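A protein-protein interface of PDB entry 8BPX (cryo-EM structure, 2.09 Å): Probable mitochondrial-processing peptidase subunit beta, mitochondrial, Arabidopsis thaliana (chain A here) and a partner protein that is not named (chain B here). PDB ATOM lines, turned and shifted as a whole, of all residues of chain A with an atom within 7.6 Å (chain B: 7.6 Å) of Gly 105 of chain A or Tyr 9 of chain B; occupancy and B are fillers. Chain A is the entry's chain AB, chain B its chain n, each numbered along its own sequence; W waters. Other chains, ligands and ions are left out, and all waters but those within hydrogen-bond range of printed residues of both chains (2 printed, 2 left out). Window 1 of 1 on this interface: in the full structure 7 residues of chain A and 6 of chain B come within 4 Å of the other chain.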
ATOM      1  N   THR A 100       4.345 -17.716  22.604  1.00  0.00           N
ATOM      2  CA  THR A 100       3.704 -16.886  21.597  1.00  0.00           C
ATOM      3  C   THR A 100       2.292 -16.542  22.044  1.00  0.00           C
ATOM      4  O   THR A 100       1.543 -17.414  22.496  1.00  0.00           O
ATOM      5  CB  THR A 100       3.676 -17.598  20.238  1.00  0.00           C
ATOM      6  OG1 THR A 100       4.954 -17.470  19.604  1.00  0.00           O
ATOM      7  CG2 THR A 100       2.613 -17.004  19.330  1.00  0.00           C
ATOM      8  N   THR A 101       1.931 -15.267  21.928  1.00  0.00           N
ATOM      9  CA  THR A 101       0.592 -14.796  22.250  1.00  0.00           C
ATOM     10  C   THR A 101      -0.178 -14.571  20.957  1.00  0.00           C
ATOM     11  O   THR A 101       0.278 -13.835  20.077  1.00  0.00           O
ATOM     12  CB  THR A 101       0.631 -13.511  23.076  1.00  0.00           C
ATOM     13  OG1 THR A 101       1.620 -13.633  24.104  1.00  0.00           O
ATOM     14  CG2 THR A 101      -0.726 -13.249  23.706  1.00  0.00           C
ATOM     15  N   LEU A 102      -1.341 -15.205  20.853  1.00  0.00           N
ATOM     16  CA  LEU A 102      -2.217 -15.040  19.712  1.00  0.00           C
ATOM     17  C   LEU A 102      -2.909 -13.681  19.790  1.00  0.00           C
ATOM     18  O   LEU A 102      -2.876 -13.017  20.828  1.00  0.00           O
ATOM     19  CB  LEU A 102      -3.230 -16.185  19.667  1.00  0.00           C
ATOM     20  CG  LEU A 102      -2.685 -17.549  19.238  1.00  0.00           C
ATOM     21  CD1 LEU A 102      -3.775 -18.390  18.594  1.00  0.00           C
ATOM     22  CD2 LEU A 102      -1.514 -17.378  18.290  1.00  0.00           C
ATOM     23  N   PRO A 103      -3.517 -13.223  18.693  1.00  0.00           N
ATOM     24  CA  PRO A 103      -4.241 -11.939  18.743  1.00  0.00           C
ATOM     25  C   PRO A 103      -5.388 -11.908  19.743  1.00  0.00           C
ATOM     26  O   PRO A 103      -5.728 -10.826  20.235  1.00  0.00           O
ATOM     27  CB  PRO A 103      -4.749 -11.766  17.306  1.00  0.00           C
ATOM     28  CG  PRO A 103      -3.834 -12.581  16.481  1.00  0.00           C
ATOM     29  CD  PRO A 103      -3.447 -13.756  17.320  1.00  0.00           C
ATOM     30  N   ASN A 104      -5.998 -13.045  20.062  1.00  0.00           N
ATOM     31  CA  ASN A 104      -7.094 -13.065  21.023  1.00  0.00           C
ATOM     32  C   ASN A 104      -6.620 -13.223  22.460  1.00  0.00           C
ATOM     33  O   ASN A 104      -7.456 -13.348  23.360  1.00  0.00           O
ATOM     34  CB  ASN A 104      -8.083 -14.184  20.680  1.00  0.00           C
ATOM     35  CG  ASN A 104      -7.409 -15.527  20.512  1.00  0.00           C
ATOM     36  OD1 ASN A 104      -6.195 -15.645  20.647  1.00  0.00           O
ATOM     37  ND2 ASN A 104      -8.194 -16.550  20.215  1.00  0.00           N
ATOM     38  N   GLY A 105      -5.313 -13.221  22.699  1.00  0.00           N
ATOM     39  CA  GLY A 105      -4.766 -13.380  24.029  1.00  0.00           C
ATOM     40  C   GLY A 105      -4.367 -14.791  24.394  1.00  0.00           C
ATOM     41  O   GLY A 105      -3.765 -14.988  25.455  1.00  0.00           O
ATOM     42  N   LEU A 106      -4.683 -15.773  23.555  1.00  0.00           N
ATOM     43  CA  LEU A 106      -4.252 -17.142  23.795  1.00  0.00           C
ATOM     44  C   LEU A 106      -2.731 -17.241  23.747  1.00  0.00           C
ATOM     45  O   LEU A 106      -2.077 -16.624  22.903  1.00  0.00           O
ATOM     46  CB  LEU A 106      -4.869 -18.074  22.756  1.00  0.00           C
ATOM     47  CG  LEU A 106      -4.938 -19.549  23.136  1.00  0.00           C
ATOM     48  CD1 LEU A 106      -5.614 -19.687  24.478  1.00  0.00           C
ATOM     49  CD2 LEU A 106      -5.675 -20.342  22.074  1.00  0.00           C
ATOM     50  N   ARG A 107      -2.164 -18.025  24.659  1.00  0.00           N
ATOM     51  CA  ARG A 107      -0.722 -18.214  24.735  1.00  0.00           C
ATOM     52  C   ARG A 107      -0.363 -19.653  24.397  1.00  0.00           C
ATOM     53  O   ARG A 107      -1.004 -20.592  24.880  1.00  0.00           O
ATOM     54  CB  ARG A 107      -0.188 -17.836  26.116  1.00  0.00           C
ATOM     55  CG  ARG A 107      -0.278 -16.353  26.423  1.00  0.00           C
ATOM     56  CD  ARG A 107       0.060 -16.055  27.869  1.00  0.00           C
ATOM     57  NE  ARG A 107      -1.078 -16.264  28.753  1.00  0.00           N
ATOM     58  CZ  ARG A 107      -0.988 -16.420  30.066  1.00  0.00           C
ATOM     59  NH1 ARG A 107       0.179 -16.393  30.686  1.00  0.00           N
ATOM     60  NH2 ARG A 107      -2.096 -16.609  30.773  1.00  0.00           N
ATOM     61  N   VAL A 108       0.652 -19.819  23.556  1.00  0.00           N
ATOM     62  CA  VAL A 108       1.177 -21.122  23.171  1.00  0.00           C
ATOM     63  C   VAL A 108       2.629 -21.181  23.615  1.00  0.00           C
ATOM     64  O   VAL A 108       3.438 -20.331  23.222  1.00  0.00           O
ATOM     65  CB  VAL A 108       1.054 -21.369  21.660  1.00  0.00           C
ATOM     66  CG1 VAL A 108       1.379 -22.811  21.331  1.00  0.00           C
ATOM     67  CG2 VAL A 108      -0.337 -21.007  21.172  1.00  0.00           C
ATOM     68  N   THR A 275     -11.885 -18.838  28.556  1.00  0.00           N
ATOM     69  CA  THR A 275     -11.629 -17.741  27.638  1.00  0.00           C
ATOM     70  C   THR A 275     -10.162 -17.723  27.228  1.00  0.00           C
ATOM     71  O   THR A 275      -9.296 -18.285  27.901  1.00  0.00           O
ATOM     72  CB  THR A 275     -12.017 -16.399  28.267  1.00  0.00           C
ATOM     73  OG1 THR A 275     -11.493 -16.325  29.596  1.00  0.00           O
ATOM     74  CG2 THR A 275     -13.527 -16.265  28.330  1.00  0.00           C
ATOM     75  N   ALA A 276      -9.893 -17.037  26.114  1.00  0.00           N
ATOM     76  CA  ALA A 276      -8.573 -17.090  25.492  1.00  0.00           C
ATOM     77  C   ALA A 276      -7.483 -16.555  26.417  1.00  0.00           C
ATOM     78  O   ALA A 276      -6.405 -17.149  26.529  1.00  0.00           O
ATOM     79  CB  ALA A 276      -8.589 -16.317  24.173  1.00  0.00           C
ATOM     80  N   SER A 277      -7.744 -15.439  27.092  1.00  0.00           N
ATOM     81  CA  SER A 277      -6.743 -14.841  27.969  1.00  0.00           C
ATOM     82  C   SER A 277      -6.519 -15.632  29.251  1.00  0.00           C
ATOM     83  O   SER A 277      -5.572 -15.332  29.985  1.00  0.00           O
ATOM     84  CB  SER A 277      -7.131 -13.405  28.323  1.00  0.00           C
ATOM     85  OG  SER A 277      -6.192 -12.829  29.210  1.00  0.00           O
ATOM     86  N   ARG A 278      -7.354 -16.623  29.541  1.00  0.00           N
ATOM     87  CA  ARG A 278      -7.201 -17.445  30.730  1.00  0.00           C
ATOM     88  C   ARG A 278      -6.652 -18.830  30.421  1.00  0.00           C
ATOM     89  O   ARG A 278      -6.559 -19.662  31.327  1.00  0.00           O
ATOM     90  CB  ARG A 278      -8.545 -17.559  31.458  1.00  0.00           C
ATOM     91  CG  ARG A 278      -8.984 -16.260  32.115  1.00  0.00           C
ATOM     92  CD  ARG A 278     -10.410 -16.319  32.644  1.00  0.00           C
ATOM     93  NE  ARG A 278     -10.557 -17.227  33.773  1.00  0.00           N
ATOM     94  CZ  ARG A 278     -11.695 -17.435  34.422  1.00  0.00           C
ATOM     95  NH1 ARG A 278     -12.806 -16.803  34.087  1.00  0.00           N
ATOM     96  NH2 ARG A 278     -11.717 -18.297  35.432  1.00  0.00           N
ATOM     97  N   MET A 279      -6.268 -19.094  29.178  1.00  0.00           N
ATOM     98  CA  MET A 279      -5.877 -20.428  28.748  1.00  0.00           C
ATOM     99  C   MET A 279      -4.463 -20.414  28.185  1.00  0.00           C
ATOM    100  O   MET A 279      -4.079 -19.493  27.458  1.00  0.00           O
ATOM    101  CB  MET A 279      -6.857 -20.970  27.707  1.00  0.00           C
ATOM    102  CG  MET A 279      -8.252 -21.211  28.246  1.00  0.00           C
ATOM    103  SD  MET A 279      -9.495 -21.412  26.952  1.00  0.00           S
ATOM    104  CE  MET A 279      -9.298 -23.142  26.558  1.00  0.00           C
ATOM    105  N   VAL A 280      -3.694 -21.440  28.532  1.00  0.00           N
ATOM    106  CA  VAL A 280      -2.344 -21.632  28.023  1.00  0.00           C
ATOM    107  C   VAL A 280      -2.267 -23.015  27.396  1.00  0.00           C
ATOM    108  O   VAL A 280      -2.631 -24.009  28.032  1.00  0.00           O
ATOM    109  CB  VAL A 280      -1.284 -21.483  29.133  1.00  0.00           C
ATOM    110  CG1 VAL A 280       0.070 -21.988  28.654  1.00  0.00           C
ATOM    111  CG2 VAL A 280      -1.185 -20.041  29.590  1.00  0.00           C
ATOM    112  N   SER A 305     -14.401 -15.378  24.745  1.00  0.00           N
ATOM    113  CA  SER A 305     -14.028 -13.966  24.773  1.00  0.00           C
ATOM    114  C   SER A 305     -14.799 -13.174  25.821  1.00  0.00           C
ATOM    115  O   SER A 305     -14.983 -11.962  25.657  1.00  0.00           O
ATOM    116  CB  SER A 305     -14.203 -13.293  23.406  1.00  0.00           C
ATOM    117  OG  SER A 305     -13.315 -13.846  22.453  1.00  0.00           O
ATOM    118  N   ASP A 306     -15.265 -13.825  26.880  1.00  0.00           N
ATOM    119  CA  ASP A 306     -15.895 -13.112  27.977  1.00  0.00           C
ATOM    120  C   ASP A 306     -14.885 -12.162  28.618  1.00  0.00           C
ATOM    121  O   ASP A 306     -13.708 -12.517  28.765  1.00  0.00           O
ATOM    122  CB  ASP A 306     -16.429 -14.105  29.013  1.00  0.00           C
ATOM    123  CG  ASP A 306     -17.467 -13.495  29.928  1.00  0.00           C
ATOM    124  OD1 ASP A 306     -18.609 -13.274  29.471  1.00  0.00           O
ATOM    125  OD2 ASP A 306     -17.142 -13.234  31.104  1.00  0.00           O
ATOM    126  N   PRO A 307     -15.293 -10.952  28.996  1.00  0.00           N
ATOM    127  CA  PRO A 307     -14.352  -9.982  29.571  1.00  0.00           C
ATOM    128  C   PRO A 307     -13.924 -10.278  30.999  1.00  0.00           C
ATOM    129  O   PRO A 307     -13.041  -9.581  31.513  1.00  0.00           O
ATOM    130  CB  PRO A 307     -15.166  -8.684  29.511  1.00  0.00           C
ATOM    131  CG  PRO A 307     -16.546  -9.159  29.765  1.00  0.00           C
ATOM    132  CD  PRO A 307     -16.650 -10.386  28.898  1.00  0.00           C
ATOM    133  N   ALA B   7     -13.442  -6.976  19.216  1.00  0.00           N
ATOM    134  CA  ALA B   7     -13.433  -8.094  20.151  1.00  0.00           C
ATOM    135  C   ALA B   7     -13.346  -7.600  21.590  1.00  0.00           C
ATOM    136  O   ALA B   7     -13.812  -6.509  21.916  1.00  0.00           O
ATOM    137  CB  ALA B   7     -12.275  -9.035  19.842  1.00  0.00           C
ATOM    138  N   ALA B   8     -12.753  -8.424  22.450  1.00  0.00           N
ATOM    139  CA  ALA B   8     -12.512  -8.081  23.845  1.00  0.00           C
ATOM    140  C   ALA B   8     -11.037  -8.016  24.196  1.00  0.00           C
ATOM    141  O   ALA B   8     -10.615  -7.097  24.899  1.00  0.00           O
ATOM    142  CB  ALA B   8     -13.206  -9.091  24.766  1.00  0.00           C
ATOM    143  N   TYR B   9     -10.240  -8.970  23.715  1.00  0.00           N
ATOM    144  CA  TYR B   9      -8.806  -8.896  23.937  1.00  0.00           C
ATOM    145  C   TYR B   9      -8.194  -7.709  23.207  1.00  0.00           C
ATOM    146  O   TYR B   9      -7.206  -7.136  23.677  1.00  0.00           O
ATOM    147  CB  TYR B   9      -8.134 -10.197  23.506  1.00  0.00           C
ATOM    148  CG  TYR B   9      -6.674 -10.266  23.874  1.00  0.00           C
ATOM    149  CD1 TYR B   9      -6.283 -10.617  25.154  1.00  0.00           C
ATOM    150  CD2 TYR B   9      -5.688  -9.980  22.942  1.00  0.00           C
ATOM    151  CE1 TYR B   9      -4.953 -10.681  25.498  1.00  0.00           C
ATOM    152  CE2 TYR B   9      -4.359 -10.043  23.275  1.00  0.00           C
ATOM    153  CZ  TYR B   9      -3.995 -10.393  24.556  1.00  0.00           C
ATOM    154  OH  TYR B   9      -2.669 -10.456  24.896  1.00  0.00           O
ATOM    155  N   PHE B  10      -8.769  -7.322  22.066  1.00  0.00           N
ATOM    156  CA  PHE B  10      -8.281  -6.147  21.355  1.00  0.00           C
ATOM    157  C   PHE B  10      -8.589  -4.865  22.123  1.00  0.00           C
ATOM    158  O   PHE B  10      -7.741  -3.971  22.205  1.00  0.00           O
ATOM    159  CB  PHE B  10      -8.887  -6.088  19.954  1.00  0.00           C
ATOM    160  CG  PHE B  10      -8.442  -4.896  19.156  1.00  0.00           C
ATOM    161  CD1 PHE B  10      -7.211  -4.887  18.527  1.00  0.00           C
ATOM    162  CD2 PHE B  10      -9.252  -3.782  19.040  1.00  0.00           C
ATOM    163  CE1 PHE B  10      -6.800  -3.798  17.797  1.00  0.00           C
ATOM    164  CE2 PHE B  10      -8.847  -2.686  18.309  1.00  0.00           C
ATOM    165  CZ  PHE B  10      -7.618  -2.693  17.687  1.00  0.00           C
ATOM    166  N   ALA B  11      -9.802  -4.748  22.668  1.00  0.00           N
ATOM    167  CA  ALA B  11     -10.153  -3.561  23.441  1.00  0.00           C
ATOM    168  C   ALA B  11      -9.372  -3.498  24.746  1.00  0.00           C
ATOM    169  O   ALA B  11      -8.913  -2.423  25.151  1.00  0.00           O
ATOM    170  CB  ALA B  11     -11.654  -3.536  23.720  1.00  0.00           C
ATOM    171  N   ARG B  12      -9.219  -4.640  25.419  1.00  0.00           N
ATOM    172  CA  ARG B  12      -8.502  -4.660  26.687  1.00  0.00           C
ATOM    173  C   ARG B  12      -7.037  -4.288  26.491  1.00  0.00           C
ATOM    174  O   ARG B  12      -6.457  -3.566  27.310  1.00  0.00           O
ATOM    175  CB  ARG B  12      -8.649  -6.035  27.339  1.00  0.00           C
ATOM    176  CG  ARG B  12      -7.517  -6.483  28.230  1.00  0.00           C
ATOM    177  CD  ARG B  12      -8.078  -7.286  29.388  1.00  0.00           C
ATOM    178  NE  ARG B  12      -7.169  -7.378  30.522  1.00  0.00           N
ATOM    179  CZ  ARG B  12      -6.395  -8.421  30.782  1.00  0.00           C
ATOM    180  NH1 ARG B  12      -6.421  -9.508  30.026  1.00  0.00           N
ATOM    181  NH2 ARG B  12      -5.572  -8.374  31.824  1.00  0.00           N
ATOM    182  N   ARG B  13      -6.470  -4.658  25.351  1.00  0.00           N
ATOM    183  CA  ARG B  13      -5.072  -4.343  24.996  1.00  0.00           C
ATOM    184  C   ARG B  13      -5.035  -2.881  24.528  1.00  0.00           C
ATOM    185  O   ARG B  13      -4.084  -2.151  24.916  1.00  0.00           O
ATOM    186  CB  ARG B  13      -4.544  -5.401  24.007  1.00  0.00           C
ATOM    187  CG  ARG B  13      -4.171  -6.723  24.655  1.00  0.00           C
ATOM    188  CD  ARG B  13      -2.802  -6.785  25.296  1.00  0.00           C
ATOM    189  NE  ARG B  13      -1.754  -6.212  24.469  1.00  0.00           N
ATOM    190  CZ  ARG B  13      -1.162  -5.057  24.713  1.00  0.00           C
ATOM    191  NH1 ARG B  13      -1.525  -4.339  25.760  1.00  0.00           N
ATOM    192  NH2 ARG B  13      -0.209  -4.622  23.914  1.00  0.00           N
ATOM    193  N   ALA B  14      -6.104  -2.438  23.894  1.00  0.00           N
ATOM    194  CA  ALA B  14      -6.168  -1.049  23.449  1.00  0.00           C
ATOM    195  C   ALA B  14      -6.248  -0.085  24.628  1.00  0.00           C
ATOM    196  O   ALA B  14      -5.602   0.970  24.622  1.00  0.00           O
ATOM    197  CB  ALA B  14      -7.361  -0.853  22.516  1.00  0.00           C
ATOM    198  N   ALA B  15      -7.037  -0.426  25.649  1.00  0.00           N
ATOM    199  CA  ALA B  15      -7.122   0.426  26.831  1.00  0.00           C
ATOM    200  C   ALA B  15      -5.775   0.524  27.534  1.00  0.00           C
ATOM    201  O   ALA B  15      -5.425   1.574  28.081  1.00  0.00           O
ATOM    202  CB  ALA B  15      -8.186  -0.106  27.788  1.00  0.00           C
ATOM    203  N   GLN B  16      -5.004  -0.566  27.519  1.00  0.00           N
ATOM    204  CA  GLN B  16      -3.670  -0.553  28.110  1.00  0.00           C
ATOM    205  C   GLN B  16      -2.735   0.373  27.342  1.00  0.00           C
ATOM    206  O   GLN B  16      -1.938   1.103  27.946  1.00  0.00           O
ATOM    207  CB  GLN B  16      -3.118  -1.977  28.137  1.00  0.00           C
ATOM    208  CG  GLN B  16      -3.584  -2.809  29.314  1.00  0.00           C
ATOM    209  CD  GLN B  16      -3.098  -4.246  29.241  1.00  0.00           C
ATOM    210  OE1 GLN B  16      -3.034  -4.837  28.164  1.00  0.00           O
ATOM    211  NE2 GLN B  16      -2.753  -4.812  30.387  1.00  0.00           N
ATOM    212  N   LYS B  17      -2.846   0.308  26.036  1.00  0.00           N
ATOM    213  CA  LYS B  17      -2.034   1.175  25.171  1.00  0.00           C
ATOM    214  C   LYS B  17      -2.282   2.641  25.526  1.00  0.00           C
ATOM    215  O   LYS B  17      -1.303   3.351  25.632  1.00  0.00           O
ATOM    216  CB  LYS B  17      -2.350   0.793  23.743  1.00  0.00           C
ATOM    217  CG  LYS B  17      -1.713  -0.486  23.229  1.00  0.00           C
ATOM    218  CD  LYS B  17      -1.956  -0.677  21.757  1.00  0.00           C
ATOM    219  CE  LYS B  17      -1.577  -2.053  21.262  1.00  0.00           C
ATOM    220  NZ  LYS B  17      -2.015  -3.096  22.213  1.00  0.00           N
ATOM    221  N   GLU B  59       4.481  -9.178  25.938  1.00  0.00           N
ATOM    222  CA  GLU B  59       3.213  -9.663  25.417  1.00  0.00           C
ATOM    223  C   GLU B  59       2.236 -10.106  26.497  1.00  0.00           C
ATOM    224  O   GLU B  59       1.025 -10.070  26.258  1.00  0.00           O
ATOM    225  CB  GLU B  59       3.447 -10.827  24.447  1.00  0.00           C
ATOM    226  CG  GLU B  59       3.562 -10.403  22.997  1.00  0.00           C
ATOM    227  CD  GLU B  59       4.695 -11.103  22.275  1.00  0.00           C
ATOM    228  OE1 GLU B  59       4.998 -12.260  22.628  1.00  0.00           O
ATOM    229  OE2 GLU B  59       5.280 -10.497  21.352  1.00  0.00           O
ATOM    230  N   ASP B  60       2.721 -10.502  27.670  1.00  0.00           N
ATOM    231  CA  ASP B  60       1.834 -10.939  28.741  1.00  0.00           C
ATOM    232  C   ASP B  60       1.016  -9.768  29.266  1.00  0.00           C
ATOM    233  O   ASP B  60       1.561  -8.710  29.594  1.00  0.00           O
ATOM    234  CB  ASP B  60       2.649 -11.570  29.869  1.00  0.00           C
ATOM    235  CG  ASP B  60       3.707 -12.525  29.354  1.00  0.00           C
ATOM    236  OD1 ASP B  60       3.400 -13.725  29.194  1.00  0.00           O
ATOM    237  OD2 ASP B  60       4.842 -12.073  29.097  1.00  0.00           O
ATOM    238  N   VAL B  61      -0.297  -9.967  29.365  1.00  0.00           N
ATOM    239  CA  VAL B  61      -1.213  -8.870  29.651  1.00  0.00           C
ATOM    240  C   VAL B  61      -1.297  -8.517  31.135  1.00  0.00           C
ATOM    241  O   VAL B  61      -1.372  -7.324  31.476  1.00  0.00           O
ATOM    242  CB  VAL B  61      -2.603  -9.205  29.074  1.00  0.00           C
ATOM    243  CG1 VAL B  61      -3.167 -10.475  29.698  1.00  0.00           C
ATOM    244  CG2 VAL B  61      -3.548  -8.033  29.216  1.00  0.00           C
ATOM    245  N   ASP B  62      -1.273  -9.510  32.030  1.00  0.00           N
ATOM    246  CA  ASP B  62      -1.252  -9.219  33.459  1.00  0.00           C
ATOM    247  C   ASP B  62       0.020  -8.477  33.843  1.00  0.00           C
ATOM    248  O   ASP B  62      -0.014  -7.539  34.651  1.00  0.00           O
ATOM    249  CB  ASP B  62      -1.372 -10.513  34.266  1.00  0.00           C
ATOM    250  CG  ASP B  62      -2.753 -11.126  34.182  1.00  0.00           C
ATOM    251  OD1 ASP B  62      -3.689 -10.425  33.747  1.00  0.00           O
ATOM    252  OD2 ASP B  62      -2.902 -12.310  34.547  1.00  0.00           O
ATOM    253  N   ILE B  64       1.618  -6.553  31.909  1.00  0.00           N
ATOM    254  CA  ILE B  64       1.466  -5.187  31.370  1.00  0.00           C
ATOM    255  C   ILE B  64       0.703  -4.399  32.424  1.00  0.00           C
ATOM    256  O   ILE B  64       1.145  -3.294  32.740  1.00  0.00           O
ATOM    257  CB  ILE B  64       0.838  -5.105  29.955  1.00  0.00           C
ATOM    258  CG1 ILE B  64       1.741  -5.683  28.867  1.00  0.00           C
ATOM    259  CG2 ILE B  64       0.404  -3.688  29.626  1.00  0.00           C
ATOM    260  CD1 ILE B  64       0.985  -6.084  27.624  1.00  0.00           C
HETATM  261  O   HOH W   1       3.381 -13.617  20.808  1.00  0.00           O
HETATM  262  O   HOH W   2       4.685 -14.430  23.935  1.00  0.00           O
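Among the printed residues, pairs that only touch across the chains: Pro 103 of chain A with Tyr 9 of chain B (2.8 Å), Gly 105 of chain A with Tyr 9 of chain B (3.1 Å), Asn 104 of chain A with Tyr 9 of chain B (3.2 Å), Thr 101 of chain A with Glu 59 of chain B (3.4 Å), Ser 305 of chain A with Ala 8 of chain B (3.5 Å), Thr 101 of chain A with Tyr 9 of chain B (3.6 Å) and Ser 277 of chain A with Val 61 of chain B (3.9 Å).
Gly 105 of chain A touches just one residue of chain B: Tyr 9 (3.1 Å). Tyr 9 of chain B touches just these residues of chain A: Thr 101 (3.6 Å), Pro 103 (2.8 Å), Asn 104 (3.2 Å) and Gly 105 (3.1 Å). Of the printed residues of chain B, Asn 104 of chain A touches Tyr 9. Of the printed residues of chain A, Arg 12 of chain B touches Ser 277. Printed residues of chain A within 4 Å of Val 61 of chain B: Ser 277. Of the printed residues of chain B, Thr 101 of chain A touches Tyr 9 (3.6 Å) and Glu 59 (3.4 Å). Ile 64 of chain B touches none of the printed residues of chain A. Ala 15 of chain B touches none of the printed residues of chain A. The nearest residue of chain A that does not touch Tyr 9 of chain B is Leu 102 of chain A (4.1 Å). The nearest printed residue of chain A that does not touch Glu 59 of chain B is Thr 100 of chain A (4.9 Å).
The guanidinium group (NH1) of Arg 12 of chain B lies within hydrogen-bond range of the side-chain hydroxyl (OG) of Ser 277 of chain A (3.4 Å).
Of the 18 printed residues of chain A, 6 touch a printed residue of chain B. Hydrophobic or aromatic side chains of chain B within 4 Å of the printed part of chain A: Ala 8, Tyr 9 and Val 61. Among the printed residues, no Asp or Glu carboxylate lies within 4 Å of a Lys or Arg side-chain nitrogen of the other chain.
Water W1 lies within hydrogen-bond range of N of Thr 101 of chain A and OE1 of Glu 59 of chain B. Water W2 bridges the side-chain carboxylate of Glu 59 of chain B and the side-chain hydroxyl of Thr 101 of chain A.
NE2 of Gln 16 of chain B is in hydrogen-bond range of O of Val 61 of chain B. OD1 of Asn 104 of chain A lies within hydrogen-bond range of N of Leu 106 of chain A, 3.3 Å away. NH2 of Arg 12 of chain B is in salt-bridge range of OD1 of Asp 62 of chain B, 3.4 Å away.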
